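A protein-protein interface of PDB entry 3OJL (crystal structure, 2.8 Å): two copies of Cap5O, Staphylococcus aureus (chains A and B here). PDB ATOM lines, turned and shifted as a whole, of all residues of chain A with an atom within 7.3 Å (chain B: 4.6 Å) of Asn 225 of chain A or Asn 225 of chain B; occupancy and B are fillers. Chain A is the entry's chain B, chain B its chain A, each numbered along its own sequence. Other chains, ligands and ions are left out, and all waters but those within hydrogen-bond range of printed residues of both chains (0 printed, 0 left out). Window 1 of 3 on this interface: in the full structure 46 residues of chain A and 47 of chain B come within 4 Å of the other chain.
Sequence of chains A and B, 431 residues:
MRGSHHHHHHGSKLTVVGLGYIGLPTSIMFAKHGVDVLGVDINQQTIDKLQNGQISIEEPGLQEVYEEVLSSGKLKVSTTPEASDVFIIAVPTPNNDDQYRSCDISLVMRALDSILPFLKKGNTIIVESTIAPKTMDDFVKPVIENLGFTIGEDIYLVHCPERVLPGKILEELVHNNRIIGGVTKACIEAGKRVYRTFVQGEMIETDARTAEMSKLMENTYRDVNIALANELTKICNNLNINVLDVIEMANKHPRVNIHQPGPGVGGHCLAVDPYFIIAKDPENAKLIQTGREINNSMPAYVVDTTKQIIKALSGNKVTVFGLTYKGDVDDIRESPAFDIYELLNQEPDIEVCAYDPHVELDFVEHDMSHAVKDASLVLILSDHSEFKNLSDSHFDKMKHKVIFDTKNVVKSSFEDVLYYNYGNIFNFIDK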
ATOM      1  N   ASN A 219       3.100   4.077 -16.455  1.00  0.00           N
ATOM      2  CA  ASN A 219       3.568   3.589 -15.160  1.00  0.00           C
ATOM      3  C   ASN A 219       4.383   4.612 -14.390  1.00  0.00           C
ATOM      4  O   ASN A 219       4.359   4.616 -13.148  1.00  0.00           O
ATOM      5  CB  ASN A 219       4.404   2.328 -15.336  1.00  0.00           C
ATOM      6  CG  ASN A 219       3.634   1.108 -15.749  1.00  0.00           C
ATOM      7  OD1 ASN A 219       2.398   1.089 -15.842  1.00  0.00           O
ATOM      8  ND2 ASN A 219       4.375   0.042 -15.978  1.00  0.00           N
ATOM      9  N   THR A 220       5.168   5.425 -15.133  1.00  0.00           N
ATOM     10  CA  THR A 220       6.035   6.473 -14.597  1.00  0.00           C
ATOM     11  C   THR A 220       5.176   7.611 -14.062  1.00  0.00           C
ATOM     12  O   THR A 220       5.366   7.986 -12.908  1.00  0.00           O
ATOM     13  CB  THR A 220       7.101   6.892 -15.624  1.00  0.00           C
ATOM     14  OG1 THR A 220       7.821   5.736 -16.009  1.00  0.00           O
ATOM     15  CG2 THR A 220       8.089   7.840 -15.048  1.00  0.00           C
ATOM     16  N   TYR A 221       4.193   8.116 -14.852  1.00  0.00           N
ATOM     17  CA  TYR A 221       3.287   9.155 -14.371  1.00  0.00           C
ATOM     18  C   TYR A 221       2.691   8.773 -12.997  1.00  0.00           C
ATOM     19  O   TYR A 221       2.648   9.603 -12.093  1.00  0.00           O
ATOM     20  CB  TYR A 221       2.160   9.437 -15.400  1.00  0.00           C
ATOM     21  CG  TYR A 221       1.042  10.333 -14.870  1.00  0.00           C
ATOM     22  CD1 TYR A 221       1.124  11.723 -14.972  1.00  0.00           C
ATOM     23  CD2 TYR A 221      -0.107   9.788 -14.302  1.00  0.00           C
ATOM     24  CE1 TYR A 221       0.098  12.540 -14.521  1.00  0.00           C
ATOM     25  CE2 TYR A 221      -1.113  10.600 -13.798  1.00  0.00           C
ATOM     26  CZ  TYR A 221      -1.009  11.979 -13.906  1.00  0.00           C
ATOM     27  OH  TYR A 221      -2.010  12.785 -13.394  1.00  0.00           O
ATOM     28  N   ARG A 222       2.210   7.519 -12.869  1.00  0.00           N
ATOM     29  CA  ARG A 222       1.595   6.933 -11.675  1.00  0.00           C
ATOM     30  C   ARG A 222       2.569   6.946 -10.480  1.00  0.00           C
ATOM     31  O   ARG A 222       2.203   7.437  -9.421  1.00  0.00           O
ATOM     32  CB  ARG A 222       1.147   5.498 -12.012  1.00  0.00           C
ATOM     33  CG  ARG A 222       0.341   4.751 -10.933  1.00  0.00           C
ATOM     34  CD  ARG A 222      -0.969   4.145 -11.457  1.00  0.00           C
ATOM     35  NE  ARG A 222      -0.798   3.202 -12.581  1.00  0.00           N
ATOM     36  CZ  ARG A 222      -1.249   3.407 -13.824  1.00  0.00           C
ATOM     37  NH1 ARG A 222      -1.903   4.525 -14.130  1.00  0.00           N
ATOM     38  NH2 ARG A 222      -1.042   2.497 -14.770  1.00  0.00           N
ATOM     39  N   ASP A 223       3.810   6.417 -10.666  1.00  0.00           N
ATOM     40  CA  ASP A 223       4.842   6.276  -9.641  1.00  0.00           C
ATOM     41  C   ASP A 223       5.301   7.619  -9.081  1.00  0.00           C
ATOM     42  O   ASP A 223       5.324   7.806  -7.860  1.00  0.00           O
ATOM     43  CB  ASP A 223       6.008   5.419 -10.180  1.00  0.00           C
ATOM     44  CG  ASP A 223       7.049   5.011  -9.151  1.00  0.00           C
ATOM     45  OD1 ASP A 223       6.679   4.335  -8.161  1.00  0.00           O
ATOM     46  OD2 ASP A 223       8.245   5.293  -9.373  1.00  0.00           O
ATOM     47  N   VAL A 224       5.626   8.560  -9.977  1.00  0.00           N
ATOM     48  CA  VAL A 224       6.062   9.918  -9.657  1.00  0.00           C
ATOM     49  C   VAL A 224       4.940  10.655  -8.905  1.00  0.00           C
ATOM     50  O   VAL A 224       5.207  11.348  -7.919  1.00  0.00           O
ATOM     51  CB  VAL A 224       6.467  10.628 -10.964  1.00  0.00           C
ATOM     52  CG1 VAL A 224       6.602  12.138 -10.768  1.00  0.00           C
ATOM     53  CG2 VAL A 224       7.749  10.017 -11.543  1.00  0.00           C
ATOM     54  N   ASN A 225       3.682  10.471  -9.362  1.00  0.00           N
ATOM     55  CA  ASN A 225       2.513  11.093  -8.758  1.00  0.00           C
ATOM     56  C   ASN A 225       2.103  10.524  -7.430  1.00  0.00           C
ATOM     57  O   ASN A 225       1.486  11.244  -6.633  1.00  0.00           O
ATOM     58  CB  ASN A 225       1.372  11.214  -9.721  1.00  0.00           C
ATOM     59  CG  ASN A 225       1.473  12.488 -10.514  1.00  0.00           C
ATOM     60  OD1 ASN A 225       1.894  12.485 -11.671  1.00  0.00           O
ATOM     61  ND2 ASN A 225       1.131  13.612  -9.891  1.00  0.00           N
ATOM     62  N   ILE A 226       2.483   9.262  -7.160  1.00  0.00           N
ATOM     63  CA  ILE A 226       2.272   8.624  -5.864  1.00  0.00           C
ATOM     64  C   ILE A 226       3.384   9.126  -4.954  1.00  0.00           C
ATOM     65  O   ILE A 226       3.099   9.415  -3.785  1.00  0.00           O
ATOM     66  CB  ILE A 226       2.224   7.081  -5.928  1.00  0.00           C
ATOM     67  CG1 ILE A 226       0.892   6.602  -6.511  1.00  0.00           C
ATOM     68  CG2 ILE A 226       2.375   6.505  -4.542  1.00  0.00           C
ATOM     69  CD1 ILE A 226       0.929   5.201  -7.042  1.00  0.00           C
ATOM     70  N   ALA A 227       4.653   9.253  -5.508  1.00  0.00           N
ATOM     71  CA  ALA A 227       5.839   9.764  -4.803  1.00  0.00           C
ATOM     72  C   ALA A 227       5.576  11.154  -4.295  1.00  0.00           C
ATOM     73  O   ALA A 227       5.941  11.436  -3.162  1.00  0.00           O
ATOM     74  CB  ALA A 227       7.053   9.760  -5.701  1.00  0.00           C
ATOM     75  N   LEU A 228       4.851  11.993  -5.079  1.00  0.00           N
ATOM     76  CA  LEU A 228       4.445  13.327  -4.649  1.00  0.00           C
ATOM     77  C   LEU A 228       3.497  13.279  -3.436  1.00  0.00           C
ATOM     78  O   LEU A 228       3.727  13.984  -2.449  1.00  0.00           O
ATOM     79  CB  LEU A 228       3.837  14.114  -5.805  1.00  0.00           C
ATOM     80  CG  LEU A 228       3.480  15.583  -5.514  1.00  0.00           C
ATOM     81  CD1 LEU A 228       4.702  16.407  -5.093  1.00  0.00           C
ATOM     82  CD2 LEU A 228       2.824  16.226  -6.723  1.00  0.00           C
ATOM     83  N   ALA A 229       2.452  12.429  -3.503  1.00  0.00           N
ATOM     84  CA  ALA A 229       1.458  12.288  -2.428  1.00  0.00           C
ATOM     85  C   ALA A 229       2.089  11.769  -1.139  1.00  0.00           C
ATOM     86  O   ALA A 229       1.695  12.183  -0.054  1.00  0.00           O
ATOM     87  CB  ALA A 229       0.335  11.368  -2.880  1.00  0.00           C
ATOM     88  N   ASN A 230       3.067  10.851  -1.271  1.00  0.00           N
ATOM     89  CA  ASN A 230       3.817  10.252  -0.169  1.00  0.00           C
ATOM     90  C   ASN A 230       4.719  11.275   0.487  1.00  0.00           C
ATOM     91  O   ASN A 230       4.738  11.346   1.701  1.00  0.00           O
ATOM     92  CB  ASN A 230       4.615   9.061  -0.649  1.00  0.00           C
ATOM     93  CG  ASN A 230       3.782   7.819  -0.848  1.00  0.00           C
ATOM     94  OD1 ASN A 230       4.084   6.970  -1.705  1.00  0.00           O
ATOM     95  ND2 ASN A 230       2.745   7.650  -0.038  1.00  0.00           N
ATOM     96  N   LEU A 232       4.276  14.559   0.315  1.00  0.00           N
ATOM     97  CA  LEU A 232       3.388  15.519   0.940  1.00  0.00           C
ATOM     98  C   LEU A 232       2.955  15.069   2.303  1.00  0.00           C
ATOM     99  O   LEU A 232       2.879  15.887   3.197  1.00  0.00           O
ATOM    100  CB  LEU A 232       2.175  15.753   0.077  1.00  0.00           C
ATOM    101  CG  LEU A 232       2.331  16.861  -0.869  1.00  0.00           C
ATOM    102  CD1 LEU A 232       1.324  16.738  -1.997  1.00  0.00           C
ATOM    103  CD2 LEU A 232       2.230  18.170  -0.115  1.00  0.00           C
ATOM    104  N   ASN A 257      -4.589  16.729 -10.358  1.00  0.00           N
ATOM    105  CA  ASN A 257      -5.036  15.346 -10.126  1.00  0.00           C
ATOM    106  C   ASN A 257      -4.014  14.589  -9.202  1.00  0.00           C
ATOM    107  O   ASN A 257      -3.525  13.500  -9.548  1.00  0.00           O
ATOM    108  CB  ASN A 257      -5.257  14.599 -11.481  1.00  0.00           C
ATOM    109  CG  ASN A 257      -5.746  15.440 -12.669  1.00  0.00           C
ATOM    110  OD1 ASN A 257      -6.945  15.694 -12.844  1.00  0.00           O
ATOM    111  ND2 ASN A 257      -4.842  15.840 -13.561  1.00  0.00           N
ATOM    112  N   ILE A 258      -3.702  15.193  -8.023  1.00  0.00           N
ATOM    113  CA  ILE A 258      -2.791  14.633  -7.016  1.00  0.00           C
ATOM    114  C   ILE A 258      -3.299  13.261  -6.650  1.00  0.00           C
ATOM    115  O   ILE A 258      -4.495  13.098  -6.436  1.00  0.00           O
ATOM    116  CB  ILE A 258      -2.631  15.544  -5.765  1.00  0.00           C
ATOM    117  CG1 ILE A 258      -2.087  16.924  -6.158  1.00  0.00           C
ATOM    118  CG2 ILE A 258      -1.766  14.890  -4.675  1.00  0.00           C
ATOM    119  CD1 ILE A 258      -2.478  18.087  -5.185  1.00  0.00           C
ATOM    120  N   HIS A 259      -2.388  12.281  -6.618  1.00  0.00           N
ATOM    121  CA  HIS A 259      -2.661  10.883  -6.307  1.00  0.00           C
ATOM    122  C   HIS A 259      -2.782  10.654  -4.798  1.00  0.00           C
ATOM    123  O   HIS A 259      -2.666  11.602  -4.008  1.00  0.00           O
ATOM    124  CB  HIS A 259      -1.592   9.977  -6.946  1.00  0.00           C
ATOM    125  CG  HIS A 259      -1.671   9.887  -8.445  1.00  0.00           C
ATOM    126  ND1 HIS A 259      -2.145  10.936  -9.215  1.00  0.00           N
ATOM    127  CD2 HIS A 259      -1.303   8.879  -9.265  1.00  0.00           C
ATOM    128  CE1 HIS A 259      -2.057  10.531 -10.464  1.00  0.00           C
ATOM    129  NE2 HIS A 259      -1.557   9.297 -10.542  1.00  0.00           N
ATOM    130  N   GLN A 260      -3.076   9.417  -4.395  1.00  0.00           N
ATOM    131  CA  GLN A 260      -3.230   9.134  -2.984  1.00  0.00           C
ATOM    132  C   GLN A 260      -1.942   8.573  -2.371  1.00  0.00           C
ATOM    133  O   GLN A 260      -1.220   7.804  -3.039  1.00  0.00           O
ATOM    134  CB  GLN A 260      -4.410   8.179  -2.745  1.00  0.00           C
ATOM    135  CG  GLN A 260      -5.767   8.869  -2.844  1.00  0.00           C
ATOM    136  CD  GLN A 260      -6.073   9.795  -1.692  1.00  0.00           C
ATOM    137  OE1 GLN A 260      -6.310  10.980  -1.864  1.00  0.00           O
ATOM    138  NE2 GLN A 260      -6.103   9.282  -0.498  1.00  0.00           N
ATOM    139  N   PRO A 261      -1.669   8.879  -1.070  1.00  0.00           N
ATOM    140  CA  PRO A 261      -0.515   8.243  -0.419  1.00  0.00           C
ATOM    141  C   PRO A 261      -0.786   6.762  -0.146  1.00  0.00           C
ATOM    142  O   PRO A 261      -1.882   6.255  -0.383  1.00  0.00           O
ATOM    143  CB  PRO A 261      -0.325   9.057   0.870  1.00  0.00           C
ATOM    144  CG  PRO A 261      -1.606   9.750   1.102  1.00  0.00           C
ATOM    145  CD  PRO A 261      -2.430   9.733  -0.130  1.00  0.00           C
ATOM    146  N   LEU A 287      14.322  12.661 -11.626  1.00  0.00           N
ATOM    147  CA  LEU A 287      12.942  12.680 -11.128  1.00  0.00           C
ATOM    148  C   LEU A 287      12.376  11.284 -10.916  1.00  0.00           C
ATOM    149  O   LEU A 287      11.796  11.043  -9.864  1.00  0.00           O
ATOM    150  CB  LEU A 287      11.996  13.546 -12.002  1.00  0.00           C
ATOM    151  CG  LEU A 287      10.683  13.954 -11.364  1.00  0.00           C
ATOM    152  CD1 LEU A 287      10.869  15.051 -10.340  1.00  0.00           C
ATOM    153  CD2 LEU A 287       9.738  14.411 -12.383  1.00  0.00           C
ATOM    154  N   GLY A 291      11.563   9.704  -7.301  1.00  0.00           N
ATOM    155  CA  GLY A 291      10.229   9.140  -7.137  1.00  0.00           C
ATOM    156  C   GLY A 291      10.251   7.724  -6.617  1.00  0.00           C
ATOM    157  O   GLY A 291       9.459   7.369  -5.736  1.00  0.00           O
ATOM    158  N   ASN A 295       9.023   6.327  -2.822  1.00  0.00           N
ATOM    159  CA  ASN A 295       8.126   5.165  -2.761  1.00  0.00           C
ATOM    160  C   ASN A 295       8.761   3.955  -2.054  1.00  0.00           C
ATOM    161  O   ASN A 295       8.075   3.244  -1.322  1.00  0.00           O
ATOM    162  CB  ASN A 295       7.571   4.812  -4.144  1.00  0.00           C
ATOM    163  CG  ASN A 295       6.587   5.844  -4.674  1.00  0.00           C
ATOM    164  OD1 ASN A 295       5.843   6.496  -3.921  1.00  0.00           O
ATOM    165  ND2 ASN A 295       6.538   6.001  -5.985  1.00  0.00           N
ATOM    166  N   TYR B 221       1.855  20.115  -8.032  1.00  0.00           N
ATOM    167  CA  TYR B 221       1.429  19.050  -8.945  1.00  0.00           C
ATOM    168  C   TYR B 221       1.837  19.398 -10.397  1.00  0.00           C
ATOM    169  O   TYR B 221       2.361  18.542 -11.106  1.00  0.00           O
ATOM    170  CB  TYR B 221      -0.095  18.792  -8.847  1.00  0.00           C
ATOM    171  CG  TYR B 221      -0.654  17.903  -9.948  1.00  0.00           C
ATOM    172  CD1 TYR B 221      -0.697  16.518  -9.803  1.00  0.00           C
ATOM    173  CD2 TYR B 221      -1.180  18.450 -11.110  1.00  0.00           C
ATOM    174  CE1 TYR B 221      -1.215  15.698 -10.803  1.00  0.00           C
ATOM    175  CE2 TYR B 221      -1.662  17.641 -12.140  1.00  0.00           C
ATOM    176  CZ  TYR B 221      -1.687  16.264 -11.981  1.00  0.00           C
ATOM    177  OH  TYR B 221      -2.180  15.488 -13.010  1.00  0.00           O
ATOM    178  N   ARG B 222       1.570  20.656 -10.826  1.00  0.00           N
ATOM    179  CA  ARG B 222       1.848  21.204 -12.151  1.00  0.00           C
ATOM    180  C   ARG B 222       3.355  21.160 -12.470  1.00  0.00           C
ATOM    181  O   ARG B 222       3.736  20.628 -13.507  1.00  0.00           O
ATOM    182  CB  ARG B 222       1.286  22.640 -12.212  1.00  0.00           C
ATOM    183  CG  ARG B 222       1.294  23.323 -13.583  1.00  0.00           C
ATOM    184  CD  ARG B 222      -0.092  23.862 -14.012  1.00  0.00           C
ATOM    185  NE  ARG B 222      -0.700  24.836 -13.082  1.00  0.00           N
ATOM    186  CZ  ARG B 222      -1.820  24.638 -12.379  1.00  0.00           C
ATOM    187  NH1 ARG B 222      -2.489  23.498 -12.487  1.00  0.00           N
ATOM    188  NH2 ARG B 222      -2.278  25.585 -11.566  1.00  0.00           N
ATOM    189  N   ASP B 223       4.201  21.703 -11.564  1.00  0.00           N
ATOM    190  CA  ASP B 223       5.653  21.818 -11.715  1.00  0.00           C
ATOM    191  C   ASP B 223       6.361  20.440 -11.817  1.00  0.00           C
ATOM    192  O   ASP B 223       7.169  20.215 -12.722  1.00  0.00           O
ATOM    193  CB  ASP B 223       6.223  22.705 -10.591  1.00  0.00           C
ATOM    194  CG  ASP B 223       7.688  23.086 -10.737  1.00  0.00           C
ATOM    195  OD1 ASP B 223       8.048  23.711 -11.773  1.00  0.00           O
ATOM    196  OD2 ASP B 223       8.469  22.805  -9.796  1.00  0.00           O
ATOM    197  N   VAL B 224       6.025  19.531 -10.909  1.00  0.00           N
ATOM    198  CA  VAL B 224       6.525  18.167 -10.850  1.00  0.00           C
ATOM    199  C   VAL B 224       6.110  17.411 -12.126  1.00  0.00           C
ATOM    200  O   VAL B 224       6.931  16.687 -12.702  1.00  0.00           O
ATOM    201  CB  VAL B 224       5.988  17.483  -9.574  1.00  0.00           C
ATOM    202  CG1 VAL B 224       6.204  15.967  -9.613  1.00  0.00           C
ATOM    203  CG2 VAL B 224       6.617  18.095  -8.327  1.00  0.00           C
ATOM    204  N   ASN B 225       4.852  17.604 -12.573  1.00  0.00           N
ATOM    205  CA  ASN B 225       4.319  16.970 -13.766  1.00  0.00           C
ATOM    206  C   ASN B 225       4.854  17.513 -15.062  1.00  0.00           C
ATOM    207  O   ASN B 225       4.852  16.783 -16.063  1.00  0.00           O
ATOM    208  CB  ASN B 225       2.827  16.878 -13.744  1.00  0.00           C
ATOM    209  CG  ASN B 225       2.360  15.638 -13.055  1.00  0.00           C
ATOM    210  OD1 ASN B 225       1.940  15.663 -11.893  1.00  0.00           O
ATOM    211  ND2 ASN B 225       2.457  14.521 -13.763  1.00  0.00           N
ATOM    212  N   ILE B 226       5.354  18.761 -15.052  1.00  0.00           N
ATOM    213  CA  ILE B 226       6.031  19.360 -16.203  1.00  0.00           C
ATOM    214  C   ILE B 226       7.469  18.828 -16.184  1.00  0.00           C
ATOM    215  O   ILE B 226       7.998  18.500 -17.250  1.00  0.00           O
ATOM    216  CB  ILE B 226       5.983  20.903 -16.220  1.00  0.00           C
ATOM    217  CG1 ILE B 226       4.590  21.397 -16.607  1.00  0.00           C
ATOM    218  CG2 ILE B 226       7.001  21.450 -17.211  1.00  0.00           C
ATOM    219  CD1 ILE B 226       4.280  22.819 -16.192  1.00  0.00           C
ATOM    220  N   ALA B 227       8.085  18.715 -14.956  1.00  0.00           N
ATOM    221  CA  ALA B 227       9.444  18.176 -14.727  1.00  0.00           C
ATOM    222  C   ALA B 227       9.533  16.768 -15.256  1.00  0.00           C
ATOM    223  O   ALA B 227      10.528  16.442 -15.896  1.00  0.00           O
ATOM    224  CB  ALA B 227       9.820  18.213 -13.257  1.00  0.00           C
ATOM    225  N   LEU B 228       8.452  15.967 -15.087  1.00  0.00           N
ATOM    226  CA  LEU B 228       8.372  14.614 -15.634  1.00  0.00           C
ATOM    227  C   LEU B 228       8.400  14.627 -17.167  1.00  0.00           C
ATOM    228  O   LEU B 228       9.196  13.888 -17.751  1.00  0.00           O
ATOM    229  CB  LEU B 228       7.125  13.874 -15.123  1.00  0.00           C
ATOM    230  CG  LEU B 228       7.002  12.389 -15.523  1.00  0.00           C
ATOM    231  CD1 LEU B 228       8.215  11.572 -15.013  1.00  0.00           C
ATOM    232  CD2 LEU B 228       5.685  11.794 -15.052  1.00  0.00           C
ATOM    233  N   ALA B 229       7.557  15.476 -17.811  1.00  0.00           N
ATOM    234  CA  ALA B 229       7.479  15.584 -19.274  1.00  0.00           C
ATOM    235  C   ALA B 229       8.796  16.043 -19.886  1.00  0.00           C
ATOM    236  O   ALA B 229       9.156  15.585 -20.966  1.00  0.00           O
ATOM    237  CB  ALA B 229       6.361  16.528 -19.675  1.00  0.00           C
ATOM    238  N   HIS B 259       1.846  15.774 -18.538  1.00  0.00           N
ATOM    239  CA  HIS B 259       1.891  17.176 -18.961  1.00  0.00           C
ATOM    240  C   HIS B 259       2.766  17.356 -20.193  1.00  0.00           C
ATOM    241  O   HIS B 259       3.313  16.383 -20.712  1.00  0.00           O
ATOM    242  CB  HIS B 259       2.327  18.084 -17.791  1.00  0.00           C
ATOM    243  CG  HIS B 259       1.317  18.206 -16.676  1.00  0.00           C
ATOM    244  ND1 HIS B 259       0.412  17.185 -16.376  1.00  0.00           N
ATOM    245  CD2 HIS B 259       1.112  19.226 -15.814  1.00  0.00           C
ATOM    246  CE1 HIS B 259      -0.298  17.619 -15.350  1.00  0.00           C
ATOM    247  NE2 HIS B 259       0.089  18.839 -14.971  1.00  0.00           N
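The side-chain amide nitrogen (ND2) of Asn 225 of chain B is in hydrogen-bond range of the side-chain amide oxygen (OD1) of Asn 225 of chain A, at 3.0 Å. The side-chain hydroxyl of Tyr 221 of chain B is in hydrogen-bond range of the side-chain amide nitrogen of Asn 257 of chain A (2.7 Å). The side-chain hydroxyl of Tyr 221 of chain A is in hydrogen-bond range of the side-chain hydroxyl of Tyr 221 of chain B.
Tyr 221 of chain B touches its own counterpart, Tyr 221 of chain A. Tyr 221 of chain A touches Asn 225 of chain B, and with the chains exchanged Asn 225 of chain A touches Tyr 221 of chain B. Val 224 of chain A touches Leu 228 of chain B, but with the chains exchanged Leu 228 of chain A does not touch Val 224 of chain B (4.1 Å). Asn 225 of chain B touches its own counterpart, Asn 225 of chain A.
Of chain A, only Tyr 221 and Asn 225 come within 4 Å of Asn 225 of chain B. Printed residues of chain B within 4 Å of Thr 220 of chain A: Leu 228 (3.7 Å). Printed residues of chain B within 4 Å of Leu 228 of chain A: Tyr 221 (3.9 Å). The nearest printed residue of chain B that does not touch Asn 225 of chain A is Leu 228 of chain B (5.1 Å). The nearest printed residue of chain B that does not touch Tyr 221 of chain A is His 259 of chain B (5.0 Å).
Along chain A the printed residues that touch a printed residue of chain B span positions 220 to 287. Among the printed residues, no Asp or Glu carboxylate lies within 4 Å of a Lys or Arg side-chain nitrogen of the other chain.
ND1 of His 259 of chain A is in hydrogen-bond range of O of Asn 257 of chain A, at 2.9 Å. The side-chain amide oxygen of Asn 225 of chain B sits close to the backbone carbonyl oxygen of Tyr 221 of chain B (3.0 Å). O of Tyr 221 of chain A sits close to OD1 of Asn 225 of chain A (3.0 Å).
Among the printed residues, merely in contact across the chains: Thr 220 of chain A with Leu 228 of chain B, Tyr 221 of chain A with Asn 225 of chain B, Tyr 221 of chain A with Leu 228 of chain B, Val 224 of chain A with Leu 228 of chain B, Asn 225 of chain A with Tyr 221 of chain B, Leu 228 of chain A with Tyr 221 of chain B, Ile 258 of chain A with Tyr 221 of chain B, Leu 287 of chain A with Val 224 of chain B, Leu 287 of chain A with Ala 227 of chain B and Leu 287 of chain A with Leu 228 of chain B.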
